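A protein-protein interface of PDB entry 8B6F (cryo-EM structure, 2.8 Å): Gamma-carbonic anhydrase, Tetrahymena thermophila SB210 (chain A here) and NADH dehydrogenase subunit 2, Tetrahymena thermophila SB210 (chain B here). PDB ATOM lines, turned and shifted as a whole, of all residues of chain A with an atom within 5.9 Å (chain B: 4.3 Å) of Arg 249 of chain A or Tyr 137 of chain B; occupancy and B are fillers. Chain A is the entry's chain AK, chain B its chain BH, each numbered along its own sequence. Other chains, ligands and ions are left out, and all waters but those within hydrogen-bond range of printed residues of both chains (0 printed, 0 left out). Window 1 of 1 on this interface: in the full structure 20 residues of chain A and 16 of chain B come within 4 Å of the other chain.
The backbone carbonyl oxygen of Tyr 137 of chain B is in hydrogen-bond range of the guanidinium group of Arg 249 of chain A (3.2 Å).
The side-chain amide nitrogen (ND2) of Asn 253 of chain A lies within hydrogen-bond range of the side-chain hydroxyl (OH) of Tyr 137 of chain B (3.4 Å).
O of Leu 255 of chain A sits at hydrogen-bond distance from OH of Tyr 137 of chain B (3.4 Å).
N of Ala 250 of chain A sits at hydrogen-bond distance from O of Ile 140 of chain B, 2.8 Å away.
The guanidinium group (NH1) of Arg 249 of chain A sits at hydrogen-bond distance from the side-chain amide oxygen (OD1) of Asn 135 of chain B, at 3.2 Å.
N of Ile 50 of chain A sits at hydrogen-bond distance from O of Tyr 136 of chain B.
NZ of Lys 256 of chain A lies close to OD1 of Asn 135 of chain B.
The backbone NH (N) of Val 138 of chain B lies within hydrogen-bond range of the backbone carbonyl oxygen (O) of Ile 50 of chain A.
The backbone carbonyl oxygen (O) of Lys 134 of chain B lies within hydrogen-bond range of the guanidinium group (NH2) of Arg 249 of chain A (2.8 Å).
The guanidinium group of Arg 249 of chain A is in hydrogen-bond range of the backbone carbonyl oxygen of Val 138 of chain B, 3.3 Å away.
The side-chain amide oxygen (OD1) of Asn 253 of chain A lies close to the backbone carbonyl oxygen (O) of Ser 54 of chain A (3.1 Å).
The guanidinium group (NH2) of Arg 210 of chain A is in hydrogen-bond range of the side-chain amide oxygen (OD1) of Asn 253 of chain A (2.6 Å).
OH of Tyr 257 of chain A lies within hydrogen-bond range of O of Leu 40 of chain A (3.3 Å).
The backbone NH of Leu 255 of chain A lies close to the side-chain amide nitrogen of Asn 253 of chain A, at 3.1 Å.
The backbone NH (N) of Asn 139 of chain B lies within hydrogen-bond range of the backbone carbonyl oxygen (O) of Asn 132 of chain B, at 2.6 Å.
The guanidinium group (NH2) of Arg 210 of chain A lies within salt-bridge range of the side-chain carboxylate (OE2) of Glu 252 of chain A (2.8 Å).
Tyr 136 of chain B touches Leu 40 of chain A (CD2 to CB, 3.4 Å).
Leu 40 of chain A touches Tyr 137 of chain B.
Pro 48 of chain A touches Tyr 136 of chain B (O to CB, 3.3 Å).
Tyr 133 of chain B touches Gln 49 of chain A.
Ile 50 of chain A touches Tyr 133 of chain B (O to CE1, 3.3 Å).
CE1 of Tyr 137 of chain B touches CG2 of Ile 50 of chain A, at 3.7 Å.
CG1 of Val 138 of chain B touches CA of Gly 51 of chain A (3.6 Å).
OD1 of Asn 139 of chain B touches CG of Arg 249 of chain A, 3.6 Å away.
Arg 249 of chain A touches Ile 140 of chain B (CA to O, 3.6 Å).
CD1 of Ile 140 of chain B touches CG of Glu 252 of chain A, 3.97 Å away.
Arg 249 of chain A touches just these residues of chain B: Lys 134, Asn 135, Tyr 137, Val 138, Asn 139 and Ile 140.
Of the printed residues of chain B, Ala 250 of chain A touches Ile 140 (2.8 Å).
Printed residues of chain A within 4 Å of Tyr 133 of chain B: Gln 49 and Ile 50.
Of the printed residues of chain A, Lys 134 of chain B touches Arg 249 (2.8 Å).
Printed residues of chain A within 4 Å of Tyr 136 of chain B: Leu 40 (3.4 Å), Pro 48 (3.3 Å), Gln 49 (3.8 Å) and Ile 50 (3.1 Å).
Of the printed residues of chain A, Tyr 137 of chain B touches Leu 40, Ile 50, Arg 249, Asn 253 and Leu 255.
The nearest printed residue of chain B that does not touch Arg 249 of chain A is Tyr 136 of chain B (5.7 Å).
The nearest printed residue of chain A that does not touch Tyr 137 of chain B is Lys 256 of chain A (4.002 Å).
The nearest printed residue of chain B that does not touch Ala 250 of chain A is Asn 139 of chain B (5.5 Å).
Hydrophobic or aromatic side chains of chain B within 4 Å of the printed part of chain A: Tyr 133, Tyr 136, Tyr 137, Val 138 and Ile 140.
Of the 20 printed residues of chain A, 11 touch a printed residue of chain B.
Printed residues of chain A that touch a printed residue of chain B: Leu 40, Pro 48, Gln 49, Ile 50, Gly 51, Arg 249, Ala 250, Glu 252, Asn 253, Leu 255 and Lys 256.
Hydrophobic or aromatic side chains of chain A that line the printed part of chain B: Leu 40, Ile 50 and Ala 250.
Among the printed residues, 21 pairs touch across the chains.
Among the printed residues, no Asp or Glu carboxylate lies within 4 Å of a Lys or Arg side-chain nitrogen of the other chain.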
ATOM      1  N   LEU A  40     -21.802  21.803   1.990  1.00  0.00           N
ATOM      2  CA  LEU A  40     -22.027  20.467   2.524  1.00  0.00           C
ATOM      3  C   LEU A  40     -23.362  20.436   3.252  1.00  0.00           C
ATOM      4  O   LEU A  40     -23.642  21.305   4.082  1.00  0.00           O
ATOM      5  CB  LEU A  40     -20.899  20.055   3.472  1.00  0.00           C
ATOM      6  CG  LEU A  40     -19.479  20.096   2.901  1.00  0.00           C
ATOM      7  CD1 LEU A  40     -18.487  19.564   3.917  1.00  0.00           C
ATOM      8  CD2 LEU A  40     -19.377  19.319   1.603  1.00  0.00           C
ATOM      9  N   PRO A  48     -22.085  13.792   4.213  1.00  0.00           N
ATOM     10  CA  PRO A  48     -20.961  13.632   3.287  1.00  0.00           C
ATOM     11  C   PRO A  48     -19.648  13.479   4.036  1.00  0.00           C
ATOM     12  O   PRO A  48     -19.464  14.016   5.131  1.00  0.00           O
ATOM     13  CB  PRO A  48     -20.993  14.922   2.459  1.00  0.00           C
ATOM     14  CG  PRO A  48     -21.697  15.902   3.310  1.00  0.00           C
ATOM     15  CD  PRO A  48     -22.707  15.123   4.093  1.00  0.00           C
ATOM     16  N   GLN A  49     -18.730  12.726   3.436  1.00  0.00           N
ATOM     17  CA  GLN A  49     -17.417  12.471   4.009  1.00  0.00           C
ATOM     18  C   GLN A  49     -16.352  12.872   3.001  1.00  0.00           C
ATOM     19  O   GLN A  49     -16.420  12.476   1.834  1.00  0.00           O
ATOM     20  CB  GLN A  49     -17.265  11.000   4.396  1.00  0.00           C
ATOM     21  CG  GLN A  49     -18.248  10.550   5.461  1.00  0.00           C
ATOM     22  CD  GLN A  49     -18.185   9.063   5.716  1.00  0.00           C
ATOM     23  OE1 GLN A  49     -17.600   8.313   4.936  1.00  0.00           O
ATOM     24  NE2 GLN A  49     -18.785   8.624   6.815  1.00  0.00           N
ATOM     25  N   ILE A  50     -15.369  13.648   3.452  1.00  0.00           N
ATOM     26  CA  ILE A  50     -14.316  14.171   2.591  1.00  0.00           C
ATOM     27  C   ILE A  50     -12.970  13.847   3.222  1.00  0.00           C
ATOM     28  O   ILE A  50     -12.785  14.031   4.429  1.00  0.00           O
ATOM     29  CB  ILE A  50     -14.464  15.690   2.363  1.00  0.00           C
ATOM     30  CG1 ILE A  50     -15.758  15.997   1.606  1.00  0.00           C
ATOM     31  CG2 ILE A  50     -13.282  16.244   1.587  1.00  0.00           C
ATOM     32  CD1 ILE A  50     -16.949  16.243   2.497  1.00  0.00           C
ATOM     33  N   GLY A  51     -12.036  13.367   2.405  1.00  0.00           N
ATOM     34  CA  GLY A  51     -10.713  13.015   2.870  1.00  0.00           C
ATOM     35  C   GLY A  51      -9.802  14.223   2.982  1.00  0.00           C
ATOM     36  O   GLY A  51     -10.208  15.374   2.809  1.00  0.00           O
ATOM     37  N   SER A  54      -8.577  17.406   0.192  1.00  0.00           N
ATOM     38  CA  SER A  54      -9.650  17.449  -0.791  1.00  0.00           C
ATOM     39  C   SER A  54     -10.319  18.815  -0.724  1.00  0.00           C
ATOM     40  O   SER A  54     -10.795  19.224   0.338  1.00  0.00           O
ATOM     41  CB  SER A  54     -10.669  16.340  -0.534  1.00  0.00           C
ATOM     42  OG  SER A  54     -10.109  15.062  -0.777  1.00  0.00           O
ATOM     43  N   ILE A  56     -13.248  21.324  -1.865  1.00  0.00           N
ATOM     44  CA  ILE A  56     -14.595  21.510  -2.389  1.00  0.00           C
ATOM     45  C   ILE A  56     -14.839  23.008  -2.488  1.00  0.00           C
ATOM     46  O   ILE A  56     -14.770  23.723  -1.482  1.00  0.00           O
ATOM     47  CB  ILE A  56     -15.658  20.831  -1.507  1.00  0.00           C
ATOM     48  CG1 ILE A  56     -15.577  19.305  -1.607  1.00  0.00           C
ATOM     49  CG2 ILE A  56     -17.061  21.281  -1.897  1.00  0.00           C
ATOM     50  CD1 ILE A  56     -14.418  18.676  -0.867  1.00  0.00           C
ATOM     51  N   ARG A 210      -6.690  26.365  -2.256  1.00  0.00           N
ATOM     52  CA  ARG A 210      -6.992  26.126  -0.850  1.00  0.00           C
ATOM     53  C   ARG A 210      -6.310  27.150   0.049  1.00  0.00           C
ATOM     54  O   ARG A 210      -6.904  27.628   1.022  1.00  0.00           O
ATOM     55  CB  ARG A 210      -6.553  24.709  -0.480  1.00  0.00           C
ATOM     56  CG  ARG A 210      -6.881  24.273   0.935  1.00  0.00           C
ATOM     57  CD  ARG A 210      -5.978  23.120   1.348  1.00  0.00           C
ATOM     58  NE  ARG A 210      -6.629  22.210   2.282  1.00  0.00           N
ATOM     59  CZ  ARG A 210      -7.399  21.192   1.926  1.00  0.00           C
ATOM     60  NH1 ARG A 210      -7.658  20.931   0.655  1.00  0.00           N
ATOM     61  NH2 ARG A 210      -7.928  20.418   2.869  1.00  0.00           N
ATOM     62  N   GLY A 245     -13.168  19.715  21.196  1.00  0.00           N
ATOM     63  CA  GLY A 245     -11.805  19.324  20.915  1.00  0.00           C
ATOM     64  C   GLY A 245     -11.193  19.995  19.709  1.00  0.00           C
ATOM     65  O   GLY A 245     -10.117  19.576  19.269  1.00  0.00           O
ATOM     66  N   ASP A 246     -11.842  21.022  19.155  1.00  0.00           N
ATOM     67  CA  ASP A 246     -11.290  21.717  17.999  1.00  0.00           C
ATOM     68  C   ASP A 246     -10.099  22.591  18.363  1.00  0.00           C
ATOM     69  O   ASP A 246      -9.363  23.013  17.466  1.00  0.00           O
ATOM     70  CB  ASP A 246     -12.366  22.560  17.318  1.00  0.00           C
ATOM     71  CG  ASP A 246     -13.230  21.744  16.375  1.00  0.00           C
ATOM     72  OD1 ASP A 246     -13.137  20.499  16.404  1.00  0.00           O
ATOM     73  OD2 ASP A 246     -13.992  22.347  15.591  1.00  0.00           O
ATOM     74  N   GLU A 247      -9.895  22.877  19.648  1.00  0.00           N
ATOM     75  CA  GLU A 247      -8.663  23.540  20.056  1.00  0.00           C
ATOM     76  C   GLU A 247      -7.458  22.624  19.893  1.00  0.00           C
ATOM     77  O   GLU A 247      -6.322  23.104  19.918  1.00  0.00           O
ATOM     78  CB  GLU A 247      -8.770  24.031  21.505  1.00  0.00           C
ATOM     79  CG  GLU A 247      -8.627  22.959  22.583  1.00  0.00           C
ATOM     80  CD  GLU A 247      -9.756  21.952  22.573  1.00  0.00           C
ATOM     81  OE1 GLU A 247     -10.740  22.168  21.835  1.00  0.00           O
ATOM     82  OE2 GLU A 247      -9.663  20.944  23.305  1.00  0.00           O
ATOM     83  N   GLU A 248      -7.689  21.319  19.730  1.00  0.00           N
ATOM     84  CA  GLU A 248      -6.634  20.359  19.446  1.00  0.00           C
ATOM     85  C   GLU A 248      -6.712  19.776  18.044  1.00  0.00           C
ATOM     86  O   GLU A 248      -5.710  19.244  17.559  1.00  0.00           O
ATOM     87  CB  GLU A 248      -6.680  19.209  20.462  1.00  0.00           C
ATOM     88  CG  GLU A 248      -6.591  19.669  21.906  1.00  0.00           C
ATOM     89  CD  GLU A 248      -6.792  18.536  22.885  1.00  0.00           C
ATOM     90  OE1 GLU A 248      -6.970  17.387  22.432  1.00  0.00           O
ATOM     91  OE2 GLU A 248      -6.775  18.793  24.107  1.00  0.00           O
ATOM     92  N   ARG A 249      -7.869  19.847  17.393  1.00  0.00           N
ATOM     93  CA  ARG A 249      -7.981  19.402  16.012  1.00  0.00           C
ATOM     94  C   ARG A 249      -7.209  20.339  15.093  1.00  0.00           C
ATOM     95  O   ARG A 249      -7.177  21.555  15.304  1.00  0.00           O
ATOM     96  CB  ARG A 249      -9.447  19.342  15.594  1.00  0.00           C
ATOM     97  CG  ARG A 249      -9.670  18.870  14.169  1.00  0.00           C
ATOM     98  CD  ARG A 249     -11.150  18.756  13.863  1.00  0.00           C
ATOM     99  NE  ARG A 249     -11.394  18.342  12.488  1.00  0.00           N
ATOM    100  CZ  ARG A 249     -12.596  18.105  11.982  1.00  0.00           C
ATOM    101  NH1 ARG A 249     -13.690  18.224  12.714  1.00  0.00           N
ATOM    102  NH2 ARG A 249     -12.703  17.737  10.709  1.00  0.00           N
ATOM    103  N   ALA A 250      -6.583  19.769  14.070  1.00  0.00           N
ATOM    104  CA  ALA A 250      -5.813  20.558  13.122  1.00  0.00           C
ATOM    105  C   ALA A 250      -6.723  21.153  12.058  1.00  0.00           C
ATOM    106  O   ALA A 250      -7.636  20.489  11.559  1.00  0.00           O
ATOM    107  CB  ALA A 250      -4.736  19.698  12.464  1.00  0.00           C
ATOM    108  N   GLN A 251      -6.469  22.414  11.708  1.00  0.00           N
ATOM    109  CA  GLN A 251      -7.229  23.098  10.663  1.00  0.00           C
ATOM    110  C   GLN A 251      -6.718  22.677   9.282  1.00  0.00           C
ATOM    111  O   GLN A 251      -6.245  23.480   8.481  1.00  0.00           O
ATOM    112  CB  GLN A 251      -7.146  24.608  10.840  1.00  0.00           C
ATOM    113  CG  GLN A 251      -7.670  25.119  12.169  1.00  0.00           C
ATOM    114  CD  GLN A 251      -6.634  25.060  13.271  1.00  0.00           C
ATOM    115  OE1 GLN A 251      -5.572  24.459  13.112  1.00  0.00           O
ATOM    116  NE2 GLN A 251      -6.936  25.695  14.397  1.00  0.00           N
ATOM    117  N   GLU A 252      -6.831  21.376   9.015  1.00  0.00           N
ATOM    118  CA  GLU A 252      -6.317  20.834   7.763  1.00  0.00           C
ATOM    119  C   GLU A 252      -7.038  21.436   6.565  1.00  0.00           C
ATOM    120  O   GLU A 252      -6.405  21.796   5.568  1.00  0.00           O
ATOM    121  CB  GLU A 252      -6.442  19.310   7.771  1.00  0.00           C
ATOM    122  CG  GLU A 252      -5.856  18.623   6.546  1.00  0.00           C
ATOM    123  CD  GLU A 252      -6.874  18.405   5.442  1.00  0.00           C
ATOM    124  OE1 GLU A 252      -8.070  18.222   5.754  1.00  0.00           O
ATOM    125  OE2 GLU A 252      -6.475  18.411   4.260  1.00  0.00           O
ATOM    126  N   ASN A 253      -8.361  21.559   6.647  1.00  0.00           N
ATOM    127  CA  ASN A 253      -9.153  22.129   5.562  1.00  0.00           C
ATOM    128  C   ASN A 253      -9.722  23.469   6.000  1.00  0.00           C
ATOM    129  O   ASN A 253     -10.543  23.509   6.930  1.00  0.00           O
ATOM    130  CB  ASN A 253     -10.279  21.177   5.162  1.00  0.00           C
ATOM    131  CG  ASN A 253     -10.881  21.527   3.819  1.00  0.00           C
ATOM    132  OD1 ASN A 253     -10.397  21.089   2.779  1.00  0.00           O
ATOM    133  ND2 ASN A 253     -11.941  22.319   3.835  1.00  0.00           N
ATOM    134  N   LEU A 255     -11.967  25.322   4.687  1.00  0.00           N
ATOM    135  CA  LEU A 255     -13.407  25.399   4.440  1.00  0.00           C
ATOM    136  C   LEU A 255     -14.178  24.403   5.299  1.00  0.00           C
ATOM    137  O   LEU A 255     -14.980  23.614   4.804  1.00  0.00           O
ATOM    138  CB  LEU A 255     -13.689  25.168   2.961  1.00  0.00           C
ATOM    139  CG  LEU A 255     -12.928  26.061   1.981  1.00  0.00           C
ATOM    140  CD1 LEU A 255     -13.244  25.661   0.552  1.00  0.00           C
ATOM    141  CD2 LEU A 255     -13.260  27.521   2.212  1.00  0.00           C
ATOM    142  N   LYS A 256     -13.946  24.444   6.608  1.00  0.00           N
ATOM    143  CA  LYS A 256     -14.580  23.537   7.554  1.00  0.00           C
ATOM    144  C   LYS A 256     -15.416  24.345   8.533  1.00  0.00           C
ATOM    145  O   LYS A 256     -14.940  25.342   9.086  1.00  0.00           O
ATOM    146  CB  LYS A 256     -13.531  22.705   8.297  1.00  0.00           C
ATOM    147  CG  LYS A 256     -14.103  21.751   9.336  1.00  0.00           C
ATOM    148  CD  LYS A 256     -14.044  22.347  10.734  1.00  0.00           C
ATOM    149  CE  LYS A 256     -14.729  21.448  11.747  1.00  0.00           C
ATOM    150  NZ  LYS A 256     -14.727  22.047  13.110  1.00  0.00           N
ATOM    151  N   TYR A 257     -16.657  23.918   8.741  1.00  0.00           N
ATOM    152  CA  TYR A 257     -17.561  24.606   9.655  1.00  0.00           C
ATOM    153  C   TYR A 257     -16.979  24.645  11.063  1.00  0.00           C
ATOM    154  O   TYR A 257     -16.833  23.610  11.711  1.00  0.00           O
ATOM    155  CB  TYR A 257     -18.929  23.922   9.676  1.00  0.00           C
ATOM    156  CG  TYR A 257     -19.624  23.875   8.332  1.00  0.00           C
ATOM    157  CD1 TYR A 257     -19.400  24.855   7.373  1.00  0.00           C
ATOM    158  CD2 TYR A 257     -20.505  22.849   8.024  1.00  0.00           C
ATOM    159  CE1 TYR A 257     -20.033  24.814   6.146  1.00  0.00           C
ATOM    160  CE2 TYR A 257     -21.143  22.797   6.800  1.00  0.00           C
ATOM    161  CZ  TYR A 257     -20.903  23.782   5.867  1.00  0.00           C
ATOM    162  OH  TYR A 257     -21.537  23.735   4.649  1.00  0.00           O
ATOM    163  N   ASN B 132     -10.983   9.216  11.021  1.00  0.00           N
ATOM    164  CA  ASN B 132     -12.375   9.430  11.390  1.00  0.00           C
ATOM    165  C   ASN B 132     -12.868  10.756  10.830  1.00  0.00           C
ATOM    166  O   ASN B 132     -12.125  11.737  10.762  1.00  0.00           O
ATOM    167  CB  ASN B 132     -12.537   9.416  12.910  1.00  0.00           C
ATOM    168  CG  ASN B 132     -12.264   8.055  13.511  1.00  0.00           C
ATOM    169  OD1 ASN B 132     -11.146   7.762  13.931  1.00  0.00           O
ATOM    170  ND2 ASN B 132     -13.289   7.212  13.552  1.00  0.00           N
ATOM    171  N   TYR B 133     -14.136  10.784  10.431  1.00  0.00           N
ATOM    172  CA  TYR B 133     -14.749  11.974   9.860  1.00  0.00           C
ATOM    173  C   TYR B 133     -15.515  12.720  10.942  1.00  0.00           C
ATOM    174  O   TYR B 133     -16.339  12.130  11.647  1.00  0.00           O
ATOM    175  CB  TYR B 133     -15.689  11.607   8.711  1.00  0.00           C
ATOM    176  CG  TYR B 133     -14.996  10.937   7.551  1.00  0.00           C
ATOM    177  CD1 TYR B 133     -14.267  11.676   6.633  1.00  0.00           C
ATOM    178  CD2 TYR B 133     -15.075   9.563   7.372  1.00  0.00           C
ATOM    179  CE1 TYR B 133     -13.632  11.068   5.571  1.00  0.00           C
ATOM    180  CE2 TYR B 133     -14.445   8.945   6.315  1.00  0.00           C
ATOM    181  CZ  TYR B 133     -13.725   9.703   5.417  1.00  0.00           C
ATOM    182  OH  TYR B 133     -13.094   9.094   4.359  1.00  0.00           O
ATOM    183  N   LYS B 134     -15.240  14.015  11.069  1.00  0.00           N
ATOM    184  CA  LYS B 134     -15.953  14.879  11.996  1.00  0.00           C
ATOM    185  C   LYS B 134     -16.264  16.184  11.286  1.00  0.00           C
ATOM    186  O   LYS B 134     -15.370  16.799  10.697  1.00  0.00           O
ATOM    187  CB  LYS B 134     -15.133  15.136  13.261  1.00  0.00           C
ATOM    188  CG  LYS B 134     -15.889  15.876  14.349  1.00  0.00           C
ATOM    189  CD  LYS B 134     -15.062  15.980  15.617  1.00  0.00           C
ATOM    190  CE  LYS B 134     -15.878  16.559  16.756  1.00  0.00           C
ATOM    191  NZ  LYS B 134     -15.099  16.608  18.024  1.00  0.00           N
ATOM    192  N   ASN B 135     -17.524  16.609  11.348  1.00  0.00           N
ATOM    193  CA  ASN B 135     -17.983  17.789  10.619  1.00  0.00           C
ATOM    194  C   ASN B 135     -17.759  17.619   9.118  1.00  0.00           C
ATOM    195  O   ASN B 135     -17.402  18.565   8.415  1.00  0.00           O
ATOM    196  CB  ASN B 135     -17.299  19.059  11.126  1.00  0.00           C
ATOM    197  CG  ASN B 135     -17.485  19.263  12.615  1.00  0.00           C
ATOM    198  OD1 ASN B 135     -16.522  19.484  13.347  1.00  0.00           O
ATOM    199  ND2 ASN B 135     -18.728  19.186  13.071  1.00  0.00           N
ATOM    200  N   TYR B 136     -17.965  16.396   8.629  1.00  0.00           N
ATOM    201  CA  TYR B 136     -17.859  16.028   7.220  1.00  0.00           C
ATOM    202  C   TYR B 136     -16.422  15.983   6.721  1.00  0.00           C
ATOM    203  O   TYR B 136     -16.202  15.784   5.522  1.00  0.00           O
ATOM    204  CB  TYR B 136     -18.662  16.978   6.324  1.00  0.00           C
ATOM    205  CG  TYR B 136     -20.099  17.179   6.751  1.00  0.00           C
ATOM    206  CD1 TYR B 136     -20.786  16.199   7.453  1.00  0.00           C
ATOM    207  CD2 TYR B 136     -20.768  18.355   6.447  1.00  0.00           C
ATOM    208  CE1 TYR B 136     -22.097  16.386   7.840  1.00  0.00           C
ATOM    209  CE2 TYR B 136     -22.078  18.551   6.831  1.00  0.00           C
ATOM    210  CZ  TYR B 136     -22.736  17.564   7.526  1.00  0.00           C
ATOM    211  OH  TYR B 136     -24.043  17.762   7.906  1.00  0.00           O
ATOM    212  N   TYR B 137     -15.436  16.156   7.598  1.00  0.00           N
ATOM    213  CA  TYR B 137     -14.035  16.157   7.211  1.00  0.00           C
ATOM    214  C   TYR B 137     -13.245  15.235   8.125  1.00  0.00           C
ATOM    215  O   TYR B 137     -13.619  15.003   9.277  1.00  0.00           O
ATOM    216  CB  TYR B 137     -13.435  17.568   7.264  1.00  0.00           C
ATOM    217  CG  TYR B 137     -13.813  18.439   6.092  1.00  0.00           C
ATOM    218  CD1 TYR B 137     -13.143  18.336   4.882  1.00  0.00           C
ATOM    219  CD2 TYR B 137     -14.832  19.376   6.199  1.00  0.00           C
ATOM    220  CE1 TYR B 137     -13.483  19.134   3.808  1.00  0.00           C
ATOM    221  CE2 TYR B 137     -15.178  20.178   5.132  1.00  0.00           C
ATOM    222  CZ  TYR B 137     -14.500  20.053   3.940  1.00  0.00           C
ATOM    223  OH  TYR B 137     -14.843  20.852   2.876  1.00  0.00           O
ATOM    224  N   VAL B 138     -12.140  14.710   7.594  1.00  0.00           N
ATOM    225  CA  VAL B 138     -11.279  13.842   8.383  1.00  0.00           C
ATOM    226  C   VAL B 138     -10.750  14.606   9.585  1.00  0.00           C
ATOM    227  O   VAL B 138     -10.356  15.775   9.484  1.00  0.00           O
ATOM    228  CB  VAL B 138     -10.128  13.293   7.523  1.00  0.00           C
ATOM    229  CG1 VAL B 138     -10.670  12.359   6.459  1.00  0.00           C
ATOM    230  CG2 VAL B 138      -9.330  14.426   6.892  1.00  0.00           C
ATOM    231  N   ASN B 139     -10.740  13.944  10.735  1.00  0.00           N
ATOM    232  CA  ASN B 139     -10.314  14.549  11.989  1.00  0.00           C
ATOM    233  C   ASN B 139      -8.852  14.190  12.229  1.00  0.00           C
ATOM    234  O   ASN B 139      -8.528  13.034  12.522  1.00  0.00           O
ATOM    235  CB  ASN B 139     -11.196  14.065  13.139  1.00  0.00           C
ATOM    236  CG  ASN B 139     -10.929  14.802  14.432  1.00  0.00           C
ATOM    237  OD1 ASN B 139      -9.835  15.319  14.654  1.00  0.00           O
ATOM    238  ND2 ASN B 139     -11.929  14.848  15.301  1.00  0.00           N
ATOM    239  N   ILE B 140      -7.975  15.184  12.109  1.00  0.00           N
ATOM    240  CA  ILE B 140      -6.551  15.031  12.377  1.00  0.00           C
ATOM    241  C   ILE B 140      -6.243  15.792  13.658  1.00  0.00           C
ATOM    242  O   ILE B 140      -6.553  16.983  13.770  1.00  0.00           O
ATOM    243  CB  ILE B 140      -5.692  15.545  11.210  1.00  0.00           C
ATOM    244  CG1 ILE B 140      -6.101  14.847   9.909  1.00  0.00           C
ATOM    245  CG2 ILE B 140      -4.215  15.315  11.503  1.00  0.00           C
ATOM    246  CD1 ILE B 140      -5.347  15.321   8.684  1.00  0.00           C
